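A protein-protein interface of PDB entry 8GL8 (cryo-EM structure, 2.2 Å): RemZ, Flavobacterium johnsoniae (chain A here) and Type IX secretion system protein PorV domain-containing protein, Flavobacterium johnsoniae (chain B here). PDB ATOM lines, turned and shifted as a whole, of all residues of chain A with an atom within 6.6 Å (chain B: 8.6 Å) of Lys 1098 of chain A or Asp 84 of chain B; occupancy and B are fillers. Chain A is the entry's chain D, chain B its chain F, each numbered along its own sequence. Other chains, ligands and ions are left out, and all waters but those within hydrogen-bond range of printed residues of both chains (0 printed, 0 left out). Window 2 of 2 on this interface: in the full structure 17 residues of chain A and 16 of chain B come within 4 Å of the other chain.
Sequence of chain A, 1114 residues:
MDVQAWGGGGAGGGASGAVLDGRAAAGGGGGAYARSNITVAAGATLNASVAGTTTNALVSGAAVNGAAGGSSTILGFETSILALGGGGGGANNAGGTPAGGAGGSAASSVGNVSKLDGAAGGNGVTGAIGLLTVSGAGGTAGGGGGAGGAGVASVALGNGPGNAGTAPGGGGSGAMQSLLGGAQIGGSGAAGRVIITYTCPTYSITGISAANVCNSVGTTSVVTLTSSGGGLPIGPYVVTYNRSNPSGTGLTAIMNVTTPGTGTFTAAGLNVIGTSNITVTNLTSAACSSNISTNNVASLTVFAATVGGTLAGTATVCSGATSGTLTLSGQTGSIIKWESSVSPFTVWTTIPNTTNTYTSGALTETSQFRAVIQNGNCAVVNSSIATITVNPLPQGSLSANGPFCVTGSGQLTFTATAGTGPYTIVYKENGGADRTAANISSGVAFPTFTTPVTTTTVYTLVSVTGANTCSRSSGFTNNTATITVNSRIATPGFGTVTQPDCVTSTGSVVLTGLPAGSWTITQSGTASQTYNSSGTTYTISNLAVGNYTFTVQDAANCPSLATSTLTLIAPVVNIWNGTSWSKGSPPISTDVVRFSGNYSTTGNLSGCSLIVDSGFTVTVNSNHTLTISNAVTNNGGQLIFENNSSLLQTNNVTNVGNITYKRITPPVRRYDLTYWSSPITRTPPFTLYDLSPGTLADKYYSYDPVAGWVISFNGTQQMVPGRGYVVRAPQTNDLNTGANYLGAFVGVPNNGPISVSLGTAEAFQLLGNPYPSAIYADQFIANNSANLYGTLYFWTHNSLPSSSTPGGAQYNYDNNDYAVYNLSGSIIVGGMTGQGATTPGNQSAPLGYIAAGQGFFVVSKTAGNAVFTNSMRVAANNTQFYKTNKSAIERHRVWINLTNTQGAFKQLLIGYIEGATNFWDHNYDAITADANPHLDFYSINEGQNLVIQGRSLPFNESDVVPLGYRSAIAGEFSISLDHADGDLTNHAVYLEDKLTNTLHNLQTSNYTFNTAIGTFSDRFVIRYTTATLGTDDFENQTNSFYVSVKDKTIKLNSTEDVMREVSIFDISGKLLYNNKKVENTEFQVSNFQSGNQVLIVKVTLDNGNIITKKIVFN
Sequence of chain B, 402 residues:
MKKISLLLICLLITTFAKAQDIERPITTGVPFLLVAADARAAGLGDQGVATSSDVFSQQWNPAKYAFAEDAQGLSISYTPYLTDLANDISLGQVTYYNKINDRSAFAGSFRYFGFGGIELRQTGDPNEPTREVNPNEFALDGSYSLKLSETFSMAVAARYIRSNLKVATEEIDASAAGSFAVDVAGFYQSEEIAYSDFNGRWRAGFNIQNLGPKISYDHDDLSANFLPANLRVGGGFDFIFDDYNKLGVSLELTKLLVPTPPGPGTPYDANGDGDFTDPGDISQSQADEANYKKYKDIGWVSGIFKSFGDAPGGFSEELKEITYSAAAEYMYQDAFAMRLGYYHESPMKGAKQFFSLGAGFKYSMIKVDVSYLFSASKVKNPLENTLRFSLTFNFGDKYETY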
ATOM      1  N   GLU A1061       3.892 -28.781  -7.974  1.00  0.00           N
ATOM      2  CA  GLU A1061       4.306 -27.452  -7.551  1.00  0.00           C
ATOM      3  C   GLU A1061       3.761 -27.153  -6.164  1.00  0.00           C
ATOM      4  O   GLU A1061       2.699 -27.645  -5.779  1.00  0.00           O
ATOM      5  CB  GLU A1061       3.832 -26.372  -8.534  1.00  0.00           C
ATOM      6  CG  GLU A1061       4.725 -25.144  -8.574  1.00  0.00           C
ATOM      7  CD  GLU A1061       3.950 -23.861  -8.802  1.00  0.00           C
ATOM      8  OE1 GLU A1061       3.267 -23.402  -7.862  1.00  0.00           O
ATOM      9  OE2 GLU A1061       4.029 -23.308  -9.919  1.00  0.00           O
ATOM     10  N   VAL A1062       4.500 -26.338  -5.416  1.00  0.00           N
ATOM     11  CA  VAL A1062       4.055 -25.837  -4.122  1.00  0.00           C
ATOM     12  C   VAL A1062       4.272 -24.331  -4.087  1.00  0.00           C
ATOM     13  O   VAL A1062       5.291 -23.824  -4.569  1.00  0.00           O
ATOM     14  CB  VAL A1062       4.777 -26.532  -2.944  1.00  0.00           C
ATOM     15  CG1 VAL A1062       6.258 -26.199  -2.930  1.00  0.00           C
ATOM     16  CG2 VAL A1062       4.129 -26.149  -1.623  1.00  0.00           C
ATOM     17  N   SER A1063       3.287 -23.613  -3.555  1.00  0.00           N
ATOM     18  CA  SER A1063       3.369 -22.172  -3.371  1.00  0.00           C
ATOM     19  C   SER A1063       2.882 -21.837  -1.971  1.00  0.00           C
ATOM     20  O   SER A1063       1.843 -22.339  -1.536  1.00  0.00           O
ATOM     21  CB  SER A1063       2.538 -21.427  -4.419  1.00  0.00           C
ATOM     22  OG  SER A1063       3.322 -21.090  -5.549  1.00  0.00           O
ATOM     23  N   ILE A1064       3.632 -21.002  -1.264  1.00  0.00           N
ATOM     24  CA  ILE A1064       3.267 -20.561   0.076  1.00  0.00           C
ATOM     25  C   ILE A1064       3.094 -19.052   0.036  1.00  0.00           C
ATOM     26  O   ILE A1064       4.028 -18.325  -0.330  1.00  0.00           O
ATOM     27  CB  ILE A1064       4.309 -20.976   1.124  1.00  0.00           C
ATOM     28  CG1 ILE A1064       4.313 -22.497   1.289  1.00  0.00           C
ATOM     29  CG2 ILE A1064       4.016 -20.311   2.457  1.00  0.00           C
ATOM     30  CD1 ILE A1064       5.687 -23.092   1.435  1.00  0.00           C
ATOM     31  N   PHE A1065       1.903 -18.594   0.417  1.00  0.00           N
ATOM     32  CA  PHE A1065       1.506 -17.197   0.419  1.00  0.00           C
ATOM     33  C   PHE A1065       1.249 -16.727   1.843  1.00  0.00           C
ATOM     34  O   PHE A1065       0.910 -17.515   2.733  1.00  0.00           O
ATOM     35  CB  PHE A1065       0.228 -16.966  -0.403  1.00  0.00           C
ATOM     36  CG  PHE A1065       0.365 -17.279  -1.861  1.00  0.00           C
ATOM     37  CD1 PHE A1065       0.191 -18.571  -2.324  1.00  0.00           C
ATOM     38  CD2 PHE A1065       0.642 -16.276  -2.772  1.00  0.00           C
ATOM     39  CE1 PHE A1065       0.306 -18.857  -3.667  1.00  0.00           C
ATOM     40  CE2 PHE A1065       0.757 -16.557  -4.117  1.00  0.00           C
ATOM     41  CZ  PHE A1065       0.589 -17.850  -4.565  1.00  0.00           C
ATOM     42  N   ILE A1096      -0.769 -19.729   3.677  1.00  0.00           N
ATOM     43  CA  ILE A1096      -1.610 -20.490   2.760  1.00  0.00           C
ATOM     44  C   ILE A1096      -0.708 -21.309   1.849  1.00  0.00           C
ATOM     45  O   ILE A1096       0.174 -20.757   1.183  1.00  0.00           O
ATOM     46  CB  ILE A1096      -2.533 -19.570   1.939  1.00  0.00           C
ATOM     47  CG1 ILE A1096      -3.508 -18.836   2.861  1.00  0.00           C
ATOM     48  CG2 ILE A1096      -3.292 -20.370   0.896  1.00  0.00           C
ATOM     49  CD1 ILE A1096      -3.972 -17.504   2.325  1.00  0.00           C
ATOM     50  N   VAL A1097      -0.931 -22.619   1.816  1.00  0.00           N
ATOM     51  CA  VAL A1097      -0.153 -23.544   1.003  1.00  0.00           C
ATOM     52  C   VAL A1097      -1.046 -24.036  -0.128  1.00  0.00           C
ATOM     53  O   VAL A1097      -2.106 -24.625   0.118  1.00  0.00           O
ATOM     54  CB  VAL A1097       0.382 -24.720   1.835  1.00  0.00           C
ATOM     55  CG1 VAL A1097       1.307 -25.588   0.996  1.00  0.00           C
ATOM     56  CG2 VAL A1097       1.097 -24.211   3.076  1.00  0.00           C
ATOM     57  N   LYS A1098      -0.614 -23.790  -1.359  1.00  0.00           N
ATOM     58  CA  LYS A1098      -1.294 -24.240  -2.565  1.00  0.00           C
ATOM     59  C   LYS A1098      -0.413 -25.279  -3.243  1.00  0.00           C
ATOM     60  O   LYS A1098       0.742 -24.996  -3.576  1.00  0.00           O
ATOM     61  CB  LYS A1098      -1.566 -23.068  -3.507  1.00  0.00           C
ATOM     62  CG  LYS A1098      -2.454 -21.990  -2.918  1.00  0.00           C
ATOM     63  CD  LYS A1098      -3.505 -21.550  -3.917  1.00  0.00           C
ATOM     64  CE  LYS A1098      -4.813 -22.272  -3.689  1.00  0.00           C
ATOM     65  NZ  LYS A1098      -5.852 -21.876  -4.673  1.00  0.00           N
ATOM     66  N   VAL A1099      -0.958 -26.471  -3.450  1.00  0.00           N
ATOM     67  CA  VAL A1099      -0.215 -27.587  -4.019  1.00  0.00           C
ATOM     68  C   VAL A1099      -0.867 -27.975  -5.336  1.00  0.00           C
ATOM     69  O   VAL A1099      -2.059 -28.301  -5.372  1.00  0.00           O
ATOM     70  CB  VAL A1099      -0.168 -28.784  -3.057  1.00  0.00           C
ATOM     71  CG1 VAL A1099       0.322 -30.015  -3.781  1.00  0.00           C
ATOM     72  CG2 VAL A1099       0.727 -28.471  -1.869  1.00  0.00           C
ATOM     73  N   THR A1100      -0.088 -27.940  -6.412  1.00  0.00           N
ATOM     74  CA  THR A1100      -0.528 -28.393  -7.725  1.00  0.00           C
ATOM     75  C   THR A1100       0.008 -29.800  -7.952  1.00  0.00           C
ATOM     76  O   THR A1100       1.226 -30.013  -7.937  1.00  0.00           O
ATOM     77  CB  THR A1100      -0.040 -27.450  -8.825  1.00  0.00           C
ATOM     78  OG1 THR A1100      -0.097 -26.096  -8.358  1.00  0.00           O
ATOM     79  CG2 THR A1100      -0.907 -27.590 -10.066  1.00  0.00           C
ATOM     80  N   ILE A1106      -5.746 -28.536  -7.514  1.00  0.00           N
ATOM     81  CA  ILE A1106      -5.060 -27.678  -6.557  1.00  0.00           C
ATOM     82  C   ILE A1106      -5.607 -27.972  -5.169  1.00  0.00           C
ATOM     83  O   ILE A1106      -6.825 -27.953  -4.957  1.00  0.00           O
ATOM     84  CB  ILE A1106      -5.226 -26.188  -6.910  1.00  0.00           C
ATOM     85  CG1 ILE A1106      -4.475 -25.861  -8.200  1.00  0.00           C
ATOM     86  CG2 ILE A1106      -4.732 -25.311  -5.771  1.00  0.00           C
ATOM     87  CD1 ILE A1106      -5.272 -25.025  -9.175  1.00  0.00           C
ATOM     88  N   ILE A1107      -4.707 -28.245  -4.229  1.00  0.00           N
ATOM     89  CA  ILE A1107      -5.049 -28.493  -2.835  1.00  0.00           C
ATOM     90  C   ILE A1107      -4.647 -27.270  -2.025  1.00  0.00           C
ATOM     91  O   ILE A1107      -3.512 -26.791  -2.136  1.00  0.00           O
ATOM     92  CB  ILE A1107      -4.360 -29.760  -2.299  1.00  0.00           C
ATOM     93  CG1 ILE A1107      -4.568 -30.926  -3.265  1.00  0.00           C
ATOM     94  CG2 ILE A1107      -4.887 -30.107  -0.916  1.00  0.00           C
ATOM     95  CD1 ILE A1107      -6.010 -31.354  -3.402  1.00  0.00           C
ATOM     96  N   THR A1108      -5.573 -26.765  -1.217  1.00  0.00           N
ATOM     97  CA  THR A1108      -5.367 -25.553  -0.437  1.00  0.00           C
ATOM     98  C   THR A1108      -5.372 -25.907   1.042  1.00  0.00           C
ATOM     99  O   THR A1108      -6.256 -26.634   1.505  1.00  0.00           O
ATOM    100  CB  THR A1108      -6.458 -24.519  -0.728  1.00  0.00           C
ATOM    101  OG1 THR A1108      -6.552 -24.308  -2.140  1.00  0.00           O
ATOM    102  CG2 THR A1108      -6.133 -23.197  -0.048  1.00  0.00           C
ATOM    103  N   LYS A1109      -4.388 -25.397   1.780  1.00  0.00           N
ATOM    104  CA  LYS A1109      -4.324 -25.639   3.215  1.00  0.00           C
ATOM    105  C   LYS A1109      -3.871 -24.379   3.934  1.00  0.00           C
ATOM    106  O   LYS A1109      -2.867 -23.772   3.558  1.00  0.00           O
ATOM    107  CB  LYS A1109      -3.375 -26.798   3.538  1.00  0.00           C
ATOM    108  CG  LYS A1109      -3.700 -27.515   4.838  1.00  0.00           C
ATOM    109  CD  LYS A1109      -4.942 -28.383   4.706  1.00  0.00           C
ATOM    110  CE  LYS A1109      -4.912 -29.218   3.437  1.00  0.00           C
ATOM    111  NZ  LYS A1109      -5.849 -30.373   3.512  1.00  0.00           N
ATOM    112  N   PRO B  80     -15.726 -11.654   0.891  1.00  0.00           N
ATOM    113  CA  PRO B  80     -14.609 -12.601   0.894  1.00  0.00           C
ATOM    114  C   PRO B  80     -13.271 -11.904   0.712  1.00  0.00           C
ATOM    115  O   PRO B  80     -13.173 -10.829   0.117  1.00  0.00           O
ATOM    116  CB  PRO B  80     -14.924 -13.522  -0.288  1.00  0.00           C
ATOM    117  CG  PRO B  80     -15.744 -12.694  -1.203  1.00  0.00           C
ATOM    118  CD  PRO B  80     -16.486 -11.684  -0.370  1.00  0.00           C
ATOM    119  N   TYR B  81     -12.229 -12.539   1.240  1.00  0.00           N
ATOM    120  CA  TYR B  81     -10.860 -12.060   1.126  1.00  0.00           C
ATOM    121  C   TYR B  81     -10.004 -13.133   0.473  1.00  0.00           C
ATOM    122  O   TYR B  81     -10.092 -14.310   0.837  1.00  0.00           O
ATOM    123  CB  TYR B  81     -10.275 -11.704   2.495  1.00  0.00           C
ATOM    124  CG  TYR B  81     -10.624 -10.321   2.984  1.00  0.00           C
ATOM    125  CD1 TYR B  81     -11.855 -10.060   3.569  1.00  0.00           C
ATOM    126  CD2 TYR B  81      -9.718  -9.276   2.869  1.00  0.00           C
ATOM    127  CE1 TYR B  81     -12.176  -8.798   4.020  1.00  0.00           C
ATOM    128  CE2 TYR B  81     -10.030  -8.010   3.318  1.00  0.00           C
ATOM    129  CZ  TYR B  81     -11.260  -7.776   3.893  1.00  0.00           C
ATOM    130  OH  TYR B  81     -11.575  -6.517   4.341  1.00  0.00           O
ATOM    131  N   LEU B  82      -9.177 -12.720  -0.484  1.00  0.00           N
ATOM    132  CA  LEU B  82      -8.260 -13.612  -1.192  1.00  0.00           C
ATOM    133  C   LEU B  82      -9.008 -14.807  -1.778  1.00  0.00           C
ATOM    134  O   LEU B  82      -8.715 -15.967  -1.486  1.00  0.00           O
ATOM    135  CB  LEU B  82      -7.132 -14.078  -0.271  1.00  0.00           C
ATOM    136  CG  LEU B  82      -6.362 -13.009   0.498  1.00  0.00           C
ATOM    137  CD1 LEU B  82      -5.792 -13.620   1.760  1.00  0.00           C
ATOM    138  CD2 LEU B  82      -5.259 -12.415  -0.360  1.00  0.00           C
ATOM    139  N   THR B  83     -10.001 -14.497  -2.614  1.00  0.00           N
ATOM    140  CA  THR B  83     -10.866 -15.541  -3.153  1.00  0.00           C
ATOM    141  C   THR B  83     -10.072 -16.554  -3.966  1.00  0.00           C
ATOM    142  O   THR B  83     -10.291 -17.765  -3.845  1.00  0.00           O
ATOM    143  CB  THR B  83     -11.972 -14.917  -4.002  1.00  0.00           C
ATOM    144  OG1 THR B  83     -11.567 -13.613  -4.435  1.00  0.00           O
ATOM    145  CG2 THR B  83     -13.253 -14.805  -3.200  1.00  0.00           C
ATOM    146  N   ASP B  84      -9.137 -16.081  -4.792  1.00  0.00           N
ATOM    147  CA  ASP B  84      -8.321 -16.995  -5.584  1.00  0.00           C
ATOM    148  C   ASP B  84      -7.416 -17.846  -4.701  1.00  0.00           C
ATOM    149  O   ASP B  84      -7.161 -19.016  -5.010  1.00  0.00           O
ATOM    150  CB  ASP B  84      -7.493 -16.208  -6.600  1.00  0.00           C
ATOM    151  CG  ASP B  84      -6.627 -15.147  -5.949  1.00  0.00           C
ATOM    152  OD1 ASP B  84      -7.083 -14.528  -4.965  1.00  0.00           O
ATOM    153  OD2 ASP B  84      -5.491 -14.933  -6.421  1.00  0.00           O
ATOM    154  N   LEU B  85      -6.924 -17.282  -3.596  1.00  0.00           N
ATOM    155  CA  LEU B  85      -5.929 -17.977  -2.786  1.00  0.00           C
ATOM    156  C   LEU B  85      -6.562 -19.007  -1.858  1.00  0.00           C
ATOM    157  O   LEU B  85      -6.098 -20.149  -1.783  1.00  0.00           O
ATOM    158  CB  LEU B  85      -5.107 -16.967  -1.984  1.00  0.00           C
ATOM    159  CG  LEU B  85      -4.014 -16.234  -2.762  1.00  0.00           C
ATOM    160  CD1 LEU B  85      -3.118 -15.449  -1.820  1.00  0.00           C
ATOM    161  CD2 LEU B  85      -3.198 -17.214  -3.590  1.00  0.00           C
ATOM    162  N   ALA B  86      -7.615 -18.630  -1.137  1.00  0.00           N
ATOM    163  CA  ALA B  86      -8.185 -19.523  -0.140  1.00  0.00           C
ATOM    164  C   ALA B  86      -9.645 -19.175   0.096  1.00  0.00           C
ATOM    165  O   ALA B  86     -10.130 -18.113  -0.298  1.00  0.00           O
ATOM    166  CB  ALA B  86      -7.401 -19.463   1.176  1.00  0.00           C
ATOM    167  N   ASN B  87     -10.345 -20.099   0.745  1.00  0.00           N
ATOM    168  CA  ASN B  87     -11.719 -19.906   1.177  1.00  0.00           C
ATOM    169  C   ASN B  87     -11.761 -19.595   2.670  1.00  0.00           C
ATOM    170  O   ASN B  87     -10.757 -19.676   3.380  1.00  0.00           O
ATOM    171  CB  ASN B  87     -12.559 -21.151   0.871  1.00  0.00           C
ATOM    172  CG  ASN B  87     -13.065 -21.180  -0.556  1.00  0.00           C
ATOM    173  OD1 ASN B  87     -13.207 -20.141  -1.198  1.00  0.00           O
ATOM    174  ND2 ASN B  87     -13.343 -22.376  -1.058  1.00  0.00           N
ATOM    175  N   LYS B 380      -1.985  -2.819  -4.399  1.00  0.00           N
ATOM    176  CA  LYS B 380      -2.977  -3.848  -4.678  1.00  0.00           C
ATOM    177  C   LYS B 380      -4.079  -3.812  -3.626  1.00  0.00           C
ATOM    178  O   LYS B 380      -3.810  -3.934  -2.427  1.00  0.00           O
ATOM    179  CB  LYS B 380      -2.312  -5.222  -4.717  1.00  0.00           C
ATOM    180  CG  LYS B 380      -3.285  -6.387  -4.690  1.00  0.00           C
ATOM    181  CD  LYS B 380      -3.698  -6.787  -6.095  1.00  0.00           C
ATOM    182  CE  LYS B 380      -4.634  -7.984  -6.079  1.00  0.00           C
ATOM    183  NZ  LYS B 380      -4.739  -8.619  -7.421  1.00  0.00           N
ATOM    184  N   PRO B 382      -6.897  -5.356  -1.467  1.00  0.00           N
ATOM    185  CA  PRO B 382      -7.216  -6.730  -1.045  1.00  0.00           C
ATOM    186  C   PRO B 382      -8.599  -7.196  -1.467  1.00  0.00           C
ATOM    187  O   PRO B 382      -8.856  -8.406  -1.456  1.00  0.00           O
ATOM    188  CB  PRO B 382      -7.090  -6.668   0.484  1.00  0.00           C
ATOM    189  CG  PRO B 382      -7.259  -5.226   0.824  1.00  0.00           C
ATOM    190  CD  PRO B 382      -6.676  -4.459  -0.321  1.00  0.00           C
ATOM    191  N   GLU B 384      -9.927  -6.640  -4.518  1.00  0.00           N
ATOM    192  CA  GLU B 384     -10.011  -6.716  -5.969  1.00  0.00           C
ATOM    193  C   GLU B 384     -10.512  -8.086  -6.407  1.00  0.00           C
ATOM    194  O   GLU B 384     -10.293  -9.097  -5.734  1.00  0.00           O
ATOM    195  CB  GLU B 384      -8.646  -6.442  -6.599  1.00  0.00           C
ATOM    196  CG  GLU B 384      -8.318  -4.976  -6.774  1.00  0.00           C
ATOM    197  CD  GLU B 384      -6.944  -4.757  -7.376  1.00  0.00           C
ATOM    198  OE1 GLU B 384      -6.814  -4.852  -8.615  1.00  0.00           O
ATOM    199  OE2 GLU B 384      -5.995  -4.487  -6.613  1.00  0.00           O
ATOM    200  N   ASN B 385     -11.193  -8.107  -7.556  1.00  0.00           N
ATOM    201  CA  ASN B 385     -11.708  -9.342  -8.150  1.00  0.00           C
ATOM    202  C   ASN B 385     -12.596 -10.099  -7.166  1.00  0.00           C
ATOM    203  O   ASN B 385     -12.623 -11.330  -7.136  1.00  0.00           O
ATOM    204  CB  ASN B 385     -10.566 -10.227  -8.653  1.00  0.00           C
ATOM    205  CG  ASN B 385      -9.678  -9.519  -9.661  1.00  0.00           C
ATOM    206  OD1 ASN B 385      -9.898  -9.605 -10.869  1.00  0.00           O
ATOM    207  ND2 ASN B 385      -8.666  -8.814  -9.168  1.00  0.00           N
ATOM    208  N   THR B 386     -13.335  -9.348  -6.353  1.00  0.00           N
ATOM    209  CA  THR B 386     -14.141  -9.902  -5.275  1.00  0.00           C
ATOM    210  C   THR B 386     -15.577  -9.429  -5.428  1.00  0.00           C
ATOM    211  O   THR B 386     -15.824  -8.238  -5.638  1.00  0.00           O
ATOM    212  CB  THR B 386     -13.582  -9.487  -3.905  1.00  0.00           C
ATOM    213  OG1 THR B 386     -12.465 -10.321  -3.570  1.00  0.00           O
ATOM    214  CG2 THR B 386     -14.641  -9.608  -2.820  1.00  0.00           C
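Of the 14 printed residues of chain A, 4 touch a printed residue of chain B. Of the 13 printed residues of chain B, 2 touch a printed residue of chain A. Hydrophobic or aromatic side chains of chain B within 4 Å of the printed part of chain A: Leu 85. Among the printed residues, no Asp or Glu carboxylate lies within 4 Å of a Lys or Arg side-chain nitrogen of the other chain.
Phe 1065 of chain A touches Leu 85 of chain B. CG2 of Ile 1096 of chain A touches O of Leu 85 of chain B, 3.9 Å away. Leu 85 of chain B touches Thr 1108 of chain A.
Val 1062 of chain A touches none of the printed residues of chain B. Of the printed residues of chain B, Phe 1065 of chain A touches Leu 85 (3.9 Å). Of the printed residues of chain B, Ile 1096 of chain A touches Leu 85. Lys 1098 of chain A touches two residues of chain B. Thr 1100 of chain A touches none of the printed residues of chain B. Printed residues of chain B within 4 Å of Thr 1108 of chain A: Leu 85. Asp 84 of chain B touches just one residue of chain A: Lys 1098. Of the printed residues of chain A, Leu 85 of chain B touches Phe 1065 (3.9 Å), Ile 1096 (3.9 Å), Lys 1098 (3.1 Å) and Thr 1108 (3.5 Å). The nearest residue of chain A that does not touch Asp 84 of chain B is Thr 1108 of chain A (6.1 Å).
The backbone NH (N) of Phe 1065 of chain A lies within hydrogen-bond range of the backbone carbonyl oxygen (O) of Ile 1096 of chain A. O of Ser 1063 of chain A is in hydrogen-bond range of N of Lys 1098 of chain A (2.9 Å).
The backbone carbonyl oxygen of Asp 84 of chain B is in hydrogen-bond range of the side-chain amino group of Lys 1098 of chain A. NZ of Lys 1098 of chain A lies close to O of Leu 85 of chain B (3.4 Å).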
